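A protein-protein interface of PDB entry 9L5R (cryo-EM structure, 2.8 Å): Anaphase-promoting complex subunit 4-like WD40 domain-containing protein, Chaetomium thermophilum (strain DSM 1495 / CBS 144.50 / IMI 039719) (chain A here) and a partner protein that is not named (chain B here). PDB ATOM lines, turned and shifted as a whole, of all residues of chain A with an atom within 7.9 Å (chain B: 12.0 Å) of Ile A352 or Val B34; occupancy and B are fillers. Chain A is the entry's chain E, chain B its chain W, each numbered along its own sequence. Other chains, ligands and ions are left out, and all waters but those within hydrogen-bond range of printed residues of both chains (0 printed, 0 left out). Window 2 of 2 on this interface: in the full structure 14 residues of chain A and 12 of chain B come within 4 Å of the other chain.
The backbone NH (N) of Gly B38 lies within hydrogen-bond range of the backbone carbonyl oxygen (O) of Leu A314 (2.7 Å).
The backbone carbonyl oxygen of Val B34 sits at hydrogen-bond distance from the side-chain hydroxyl of Thr B37 (3.0 Å). The side-chain amide nitrogen of Asn B40 is in hydrogen-bond range of the backbone carbonyl oxygen of Val B34 (2.5 Å). OH of Tyr A315 sits at hydrogen-bond distance from O of Ile A352 (3.1 Å).
Among the printed residues, pairs that only touch across the chains: Leu A314 with Thr B37, Tyr A315 with Tyr B36, Leu A317 with Tyr B36 and Ile A352 with Val B34.
No residue of chain B comes within 4 Å of Thr A46. Of the printed residues of chain B, Tyr A315 touches Tyr B36. Printed residues of chain B within 4 Å of Leu A317: Tyr B36 (3.6 Å). Pro A335 touches none of the printed residues of chain B. Glu A350 touches none of the printed residues of chain B. No residue of chain B comes within 4 Å of Leu A351. Of chain B, only Val B34 (3.7 Å) comes within 4 Å of Ile A352. Of chain A, only Ile A352 (3.7 Å) comes within 4 Å of Val B34. No residue of chain A comes within 4 Å of Pro B35. Of the printed residues of chain A, Tyr B36 touches Tyr A315 and Leu A317. Printed residues of chain A within 4 Å of Thr B37: Leu A314. Of the printed residues of chain A, Gly B38 touches Leu A314 (2.7 Å). Arg B43 touches none of the printed residues of chain A. The nearest residue of chain B that does not touch Ile A352 is Thr B37 (5.9 Å).
Of the 10 printed residues of chain B, 4 touch a printed residue of chain A. Printed residues of chain B that touch a printed residue of chain A: Val B34, Tyr B36, Thr B37 and Gly B38. Hydrophobic or aromatic side chains of chain B within 4 Å of the printed part of chain A: Val B34 and Tyr B36. Among the printed residues, no Asp or Glu carboxylate lies within 4 Å of a Lys or Arg side-chain nitrogen of the other chain.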
ATOM      1  N   THR A  43     -27.852   7.529   5.764  1.00  0.00           N
ATOM      2  CA  THR A  43     -28.040   7.551   7.211  1.00  0.00           C
ATOM      3  C   THR A  43     -26.992   6.656   7.891  1.00  0.00           C
ATOM      4  O   THR A  43     -27.300   5.548   8.327  1.00  0.00           O
ATOM      5  CB  THR A  43     -29.463   7.095   7.579  1.00  0.00           C
ATOM      6  OG1 THR A  43     -30.398   7.701   6.679  1.00  0.00           O
ATOM      7  CG2 THR A  43     -29.818   7.520   8.985  1.00  0.00           C
ATOM      8  N   PRO A  44     -25.740   7.138   7.973  1.00  0.00           N
ATOM      9  CA  PRO A  44     -24.641   6.271   8.419  1.00  0.00           C
ATOM     10  C   PRO A  44     -24.492   6.165   9.927  1.00  0.00           C
ATOM     11  O   PRO A  44     -25.308   6.685  10.694  1.00  0.00           O
ATOM     12  CB  PRO A  44     -23.413   6.936   7.792  1.00  0.00           C
ATOM     13  CG  PRO A  44     -23.760   8.382   7.823  1.00  0.00           C
ATOM     14  CD  PRO A  44     -25.239   8.451   7.520  1.00  0.00           C
ATOM     15  N   ARG A  45     -23.431   5.479  10.350  1.00  0.00           N
ATOM     16  CA  ARG A  45     -23.099   5.259  11.754  1.00  0.00           C
ATOM     17  C   ARG A  45     -21.822   6.029  12.066  1.00  0.00           C
ATOM     18  O   ARG A  45     -20.773   5.759  11.472  1.00  0.00           O
ATOM     19  CB  ARG A  45     -22.926   3.769  12.026  1.00  0.00           C
ATOM     20  CG  ARG A  45     -22.782   3.404  13.476  1.00  0.00           C
ATOM     21  CD  ARG A  45     -23.916   3.970  14.291  1.00  0.00           C
ATOM     22  NE  ARG A  45     -24.203   3.125  15.440  1.00  0.00           N
ATOM     23  CZ  ARG A  45     -24.780   3.550  16.551  1.00  0.00           C
ATOM     24  NH1 ARG A  45     -25.097   4.822  16.718  1.00  0.00           N
ATOM     25  NH2 ARG A  45     -25.036   2.680  17.520  1.00  0.00           N
ATOM     26  N   THR A  46     -21.904   6.988  12.993  1.00  0.00           N
ATOM     27  CA  THR A  46     -20.799   7.908  13.241  1.00  0.00           C
ATOM     28  C   THR A  46     -20.290   7.874  14.680  1.00  0.00           C
ATOM     29  O   THR A  46     -19.580   8.797  15.091  1.00  0.00           O
ATOM     30  CB  THR A  46     -21.196   9.341  12.875  1.00  0.00           C
ATOM     31  OG1 THR A  46     -22.233   9.792  13.750  1.00  0.00           O
ATOM     32  CG2 THR A  46     -21.672   9.430  11.437  1.00  0.00           C
ATOM     33  N   SER A  47     -20.618   6.840  15.452  1.00  0.00           N
ATOM     34  CA  SER A  47     -20.098   6.737  16.811  1.00  0.00           C
ATOM     35  C   SER A  47     -20.180   5.297  17.287  1.00  0.00           C
ATOM     36  O   SER A  47     -20.836   4.454  16.672  1.00  0.00           O
ATOM     37  CB  SER A  47     -20.851   7.642  17.788  1.00  0.00           C
ATOM     38  OG  SER A  47     -20.492   7.325  19.117  1.00  0.00           O
ATOM     39  N   PRO A  52     -28.064   5.284  17.660  1.00  0.00           N
ATOM     40  CA  PRO A  52     -27.831   6.684  17.265  1.00  0.00           C
ATOM     41  C   PRO A  52     -28.432   7.700  18.217  1.00  0.00           C
ATOM     42  O   PRO A  52     -28.010   8.863  18.204  1.00  0.00           O
ATOM     43  CB  PRO A  52     -28.481   6.771  15.877  1.00  0.00           C
ATOM     44  CG  PRO A  52     -29.342   5.554  15.762  1.00  0.00           C
ATOM     45  CD  PRO A  52     -28.667   4.505  16.570  1.00  0.00           C
ATOM     46  N   LEU A 314     -27.834  24.908  12.006  1.00  0.00           N
ATOM     47  CA  LEU A 314     -27.447  23.591  11.517  1.00  0.00           C
ATOM     48  C   LEU A 314     -28.482  22.532  11.874  1.00  0.00           C
ATOM     49  O   LEU A 314     -28.846  21.706  11.031  1.00  0.00           O
ATOM     50  CB  LEU A 314     -26.079  23.210  12.077  1.00  0.00           C
ATOM     51  CG  LEU A 314     -24.884  23.361  11.139  1.00  0.00           C
ATOM     52  CD1 LEU A 314     -24.701  24.810  10.749  1.00  0.00           C
ATOM     53  CD2 LEU A 314     -23.627  22.830  11.793  1.00  0.00           C
ATOM     54  N   TYR A 315     -28.966  22.535  13.115  1.00  0.00           N
ATOM     55  CA  TYR A 315     -29.926  21.547  13.585  1.00  0.00           C
ATOM     56  C   TYR A 315     -30.948  22.224  14.481  1.00  0.00           C
ATOM     57  O   TYR A 315     -30.700  23.291  15.042  1.00  0.00           O
ATOM     58  CB  TYR A 315     -29.258  20.418  14.375  1.00  0.00           C
ATOM     59  CG  TYR A 315     -28.325  19.524  13.599  1.00  0.00           C
ATOM     60  CD1 TYR A 315     -27.002  19.880  13.390  1.00  0.00           C
ATOM     61  CD2 TYR A 315     -28.757  18.303  13.109  1.00  0.00           C
ATOM     62  CE1 TYR A 315     -26.145  19.056  12.696  1.00  0.00           C
ATOM     63  CE2 TYR A 315     -27.906  17.471  12.418  1.00  0.00           C
ATOM     64  CZ  TYR A 315     -26.603  17.854  12.214  1.00  0.00           C
ATOM     65  OH  TYR A 315     -25.751  17.026  11.522  1.00  0.00           O
ATOM     66  N   LEU A 317     -32.856  19.862  16.722  1.00  0.00           N
ATOM     67  CA  LEU A 317     -33.215  18.512  17.143  1.00  0.00           C
ATOM     68  C   LEU A 317     -34.298  18.521  18.224  1.00  0.00           C
ATOM     69  O   LEU A 317     -34.163  19.236  19.224  1.00  0.00           O
ATOM     70  CB  LEU A 317     -31.965  17.820  17.676  1.00  0.00           C
ATOM     71  CG  LEU A 317     -30.808  17.522  16.723  1.00  0.00           C
ATOM     72  CD1 LEU A 317     -29.637  16.976  17.500  1.00  0.00           C
ATOM     73  CD2 LEU A 317     -31.210  16.537  15.664  1.00  0.00           C
ATOM     74  N   PRO A 335     -19.145  13.378  17.446  1.00  0.00           N
ATOM     75  CA  PRO A 335     -20.349  14.152  17.109  1.00  0.00           C
ATOM     76  C   PRO A 335     -21.485  13.947  18.100  1.00  0.00           C
ATOM     77  O   PRO A 335     -22.649  14.177  17.766  1.00  0.00           O
ATOM     78  CB  PRO A 335     -20.727  13.625  15.717  1.00  0.00           C
ATOM     79  CG  PRO A 335     -19.530  12.874  15.233  1.00  0.00           C
ATOM     80  CD  PRO A 335     -18.903  12.315  16.460  1.00  0.00           C
ATOM     81  N   ILE A 336     -21.168  13.465  19.294  1.00  0.00           N
ATOM     82  CA  ILE A 336     -22.172  13.147  20.299  1.00  0.00           C
ATOM     83  C   ILE A 336     -22.673  14.437  20.937  1.00  0.00           C
ATOM     84  O   ILE A 336     -21.882  15.277  21.385  1.00  0.00           O
ATOM     85  CB  ILE A 336     -21.590  12.188  21.348  1.00  0.00           C
ATOM     86  CG1 ILE A 336     -21.583  10.760  20.809  1.00  0.00           C
ATOM     87  CG2 ILE A 336     -22.378  12.247  22.640  1.00  0.00           C
ATOM     88  CD1 ILE A 336     -21.135   9.732  21.818  1.00  0.00           C
ATOM     89  N   GLY A 349     -27.413  11.616  21.695  1.00  0.00           N
ATOM     90  CA  GLY A 349     -27.465  11.241  20.301  1.00  0.00           C
ATOM     91  C   GLY A 349     -26.156  11.527  19.584  1.00  0.00           C
ATOM     92  O   GLY A 349     -25.242  12.148  20.129  1.00  0.00           O
ATOM     93  N   GLU A 350     -26.084  11.062  18.341  1.00  0.00           N
ATOM     94  CA  GLU A 350     -24.943  11.311  17.471  1.00  0.00           C
ATOM     95  C   GLU A 350     -25.374  12.215  16.327  1.00  0.00           C
ATOM     96  O   GLU A 350     -26.543  12.203  15.927  1.00  0.00           O
ATOM     97  CB  GLU A 350     -24.359  10.002  16.933  1.00  0.00           C
ATOM     98  CG  GLU A 350     -25.290   9.233  16.027  1.00  0.00           C
ATOM     99  CD  GLU A 350     -24.699   7.923  15.568  1.00  0.00           C
ATOM    100  OE1 GLU A 350     -23.574   7.601  15.993  1.00  0.00           O
ATOM    101  OE2 GLU A 350     -25.353   7.217  14.776  1.00  0.00           O
ATOM    102  N   LEU A 351     -24.437  13.014  15.818  1.00  0.00           N
ATOM    103  CA  LEU A 351     -24.721  13.963  14.746  1.00  0.00           C
ATOM    104  C   LEU A 351     -24.207  13.387  13.429  1.00  0.00           C
ATOM    105  O   LEU A 351     -23.111  13.690  12.961  1.00  0.00           O
ATOM    106  CB  LEU A 351     -24.096  15.315  15.063  1.00  0.00           C
ATOM    107  CG  LEU A 351     -24.805  16.141  16.135  1.00  0.00           C
ATOM    108  CD1 LEU A 351     -24.310  17.570  16.111  1.00  0.00           C
ATOM    109  CD2 LEU A 351     -26.308  16.098  15.948  1.00  0.00           C
ATOM    110  N   ILE A 352     -25.034  12.544  12.824  1.00  0.00           N
ATOM    111  CA  ILE A 352     -24.730  11.929  11.539  1.00  0.00           C
ATOM    112  C   ILE A 352     -24.940  12.912  10.392  1.00  0.00           C
ATOM    113  O   ILE A 352     -25.270  14.078  10.594  1.00  0.00           O
ATOM    114  CB  ILE A 352     -25.580  10.657  11.333  1.00  0.00           C
ATOM    115  CG1 ILE A 352     -27.066  10.993  11.393  1.00  0.00           C
ATOM    116  CG2 ILE A 352     -25.249   9.601  12.365  1.00  0.00           C
ATOM    117  CD1 ILE A 352     -27.940   9.843  11.036  1.00  0.00           C
ATOM    118  OXT ILE A 352     -24.780  12.558   9.226  1.00  0.00           O
ATOM    119  N   VAL B  34     -30.676  13.647  10.704  1.00  0.00           N
ATOM    120  CA  VAL B  34     -30.852  13.851   9.265  1.00  0.00           C
ATOM    121  C   VAL B  34     -32.187  14.548   8.886  1.00  0.00           C
ATOM    122  O   VAL B  34     -32.148  15.507   8.117  1.00  0.00           O
ATOM    123  CB  VAL B  34     -30.659  12.507   8.495  1.00  0.00           C
ATOM    124  CG1 VAL B  34     -31.253  12.579   7.101  1.00  0.00           C
ATOM    125  CG2 VAL B  34     -29.189  12.158   8.417  1.00  0.00           C
ATOM    126  N   PRO B  35     -33.356  14.120   9.404  1.00  0.00           N
ATOM    127  CA  PRO B  35     -34.572  14.901   9.127  1.00  0.00           C
ATOM    128  C   PRO B  35     -34.591  16.247   9.810  1.00  0.00           C
ATOM    129  O   PRO B  35     -35.388  17.107   9.425  1.00  0.00           O
ATOM    130  CB  PRO B  35     -35.700  14.010   9.660  1.00  0.00           C
ATOM    131  CG  PRO B  35     -35.116  12.679   9.782  1.00  0.00           C
ATOM    132  CD  PRO B  35     -33.714  12.916  10.179  1.00  0.00           C
ATOM    133  N   TYR B  36     -33.757  16.448  10.824  1.00  0.00           N
ATOM    134  CA  TYR B  36     -33.772  17.653  11.633  1.00  0.00           C
ATOM    135  C   TYR B  36     -32.659  18.612  11.253  1.00  0.00           C
ATOM    136  O   TYR B  36     -32.410  19.576  11.981  1.00  0.00           O
ATOM    137  CB  TYR B  36     -33.665  17.285  13.107  1.00  0.00           C
ATOM    138  CG  TYR B  36     -34.426  16.037  13.476  1.00  0.00           C
ATOM    139  CD1 TYR B  36     -35.808  16.029  13.518  1.00  0.00           C
ATOM    140  CD2 TYR B  36     -33.756  14.861  13.764  1.00  0.00           C
ATOM    141  CE1 TYR B  36     -36.501  14.890  13.852  1.00  0.00           C
ATOM    142  CE2 TYR B  36     -34.438  13.720  14.095  1.00  0.00           C
ATOM    143  CZ  TYR B  36     -35.809  13.740  14.137  1.00  0.00           C
ATOM    144  OH  TYR B  36     -36.492  12.600  14.470  1.00  0.00           O
ATOM    145  N   THR B  37     -31.972  18.349  10.145  1.00  0.00           N
ATOM    146  CA  THR B  37     -30.980  19.268   9.612  1.00  0.00           C
ATOM    147  C   THR B  37     -31.660  20.575   9.215  1.00  0.00           C
ATOM    148  O   THR B  37     -32.834  20.592   8.837  1.00  0.00           O
ATOM    149  CB  THR B  37     -30.278  18.623   8.411  1.00  0.00           C
ATOM    150  OG1 THR B  37     -29.831  17.314   8.775  1.00  0.00           O
ATOM    151  CG2 THR B  37     -29.069  19.421   7.970  1.00  0.00           C
ATOM    152  N   GLY B  38     -30.921  21.681   9.353  1.00  0.00           N
ATOM    153  CA  GLY B  38     -31.481  22.992   9.069  1.00  0.00           C
ATOM    154  C   GLY B  38     -31.969  23.155   7.644  1.00  0.00           C
ATOM    155  O   GLY B  38     -32.977  23.820   7.409  1.00  0.00           O
ATOM    156  N   GLU B  39     -31.285  22.528   6.682  1.00  0.00           N
ATOM    157  CA  GLU B  39     -31.748  22.563   5.297  1.00  0.00           C
ATOM    158  C   GLU B  39     -33.073  21.829   5.131  1.00  0.00           C
ATOM    159  O   GLU B  39     -33.987  22.328   4.458  1.00  0.00           O
ATOM    160  CB  GLU B  39     -30.692  21.950   4.380  1.00  0.00           C
ATOM    161  CG  GLU B  39     -31.052  22.014   2.907  1.00  0.00           C
ATOM    162  CD  GLU B  39     -29.971  21.445   2.010  1.00  0.00           C
ATOM    163  OE1 GLU B  39     -28.943  20.977   2.539  1.00  0.00           O
ATOM    164  OE2 GLU B  39     -30.151  21.467   0.776  1.00  0.00           O
ATOM    165  N   ASN B  40     -33.193  20.646   5.739  1.00  0.00           N
ATOM    166  CA  ASN B  40     -34.420  19.865   5.639  1.00  0.00           C
ATOM    167  C   ASN B  40     -35.585  20.565   6.318  1.00  0.00           C
ATOM    168  O   ASN B  40     -36.721  20.480   5.842  1.00  0.00           O
ATOM    169  CB  ASN B  40     -34.216  18.484   6.248  1.00  0.00           C
ATOM    170  CG  ASN B  40     -33.271  17.636   5.442  1.00  0.00           C
ATOM    171  OD1 ASN B  40     -32.779  18.062   4.400  1.00  0.00           O
ATOM    172  ND2 ASN B  40     -33.005  16.430   5.919  1.00  0.00           N
ATOM    173  N   LEU B  41     -35.329  21.250   7.427  1.00  0.00           N
ATOM    174  CA  LEU B  41     -36.392  22.012   8.062  1.00  0.00           C
ATOM    175  C   LEU B  41     -36.702  23.291   7.301  1.00  0.00           C
ATOM    176  O   LEU B  41     -37.833  23.783   7.365  1.00  0.00           O
ATOM    177  CB  LEU B  41     -36.021  22.329   9.508  1.00  0.00           C
ATOM    178  CG  LEU B  41     -35.667  21.132  10.389  1.00  0.00           C
ATOM    179  CD1 LEU B  41     -35.552  21.576  11.818  1.00  0.00           C
ATOM    180  CD2 LEU B  41     -36.702  20.031  10.262  1.00  0.00           C
ATOM    181  N   ALA B  42     -35.721  23.840   6.585  1.00  0.00           N
ATOM    182  CA  ALA B  42     -35.938  25.070   5.839  1.00  0.00           C
ATOM    183  C   ALA B  42     -36.755  24.840   4.582  1.00  0.00           C
ATOM    184  O   ALA B  42     -37.529  25.717   4.188  1.00  0.00           O
ATOM    185  CB  ALA B  42     -34.598  25.707   5.472  1.00  0.00           C
ATOM    186  N   ARG B  43     -36.585  23.693   3.941  1.00  0.00           N
ATOM    187  CA  ARG B  43     -37.330  23.431   2.714  1.00  0.00           C
ATOM    188  C   ARG B  43     -38.810  23.210   3.027  1.00  0.00           C
ATOM    189  O   ARG B  43     -39.149  22.406   3.903  1.00  0.00           O
ATOM    190  CB  ARG B  43     -36.713  22.254   1.945  1.00  0.00           C
ATOM    191  CG  ARG B  43     -36.798  20.882   2.577  1.00  0.00           C
ATOM    192  CD  ARG B  43     -36.145  19.833   1.701  1.00  0.00           C
ATOM    193  NE  ARG B  43     -34.711  20.045   1.551  1.00  0.00           N
ATOM    194  CZ  ARG B  43     -34.134  20.465   0.434  1.00  0.00           C
ATOM    195  NH1 ARG B  43     -34.840  20.732  -0.651  1.00  0.00           N
ATOM    196  NH2 ARG B  43     -32.813  20.619   0.404  1.00  0.00           N
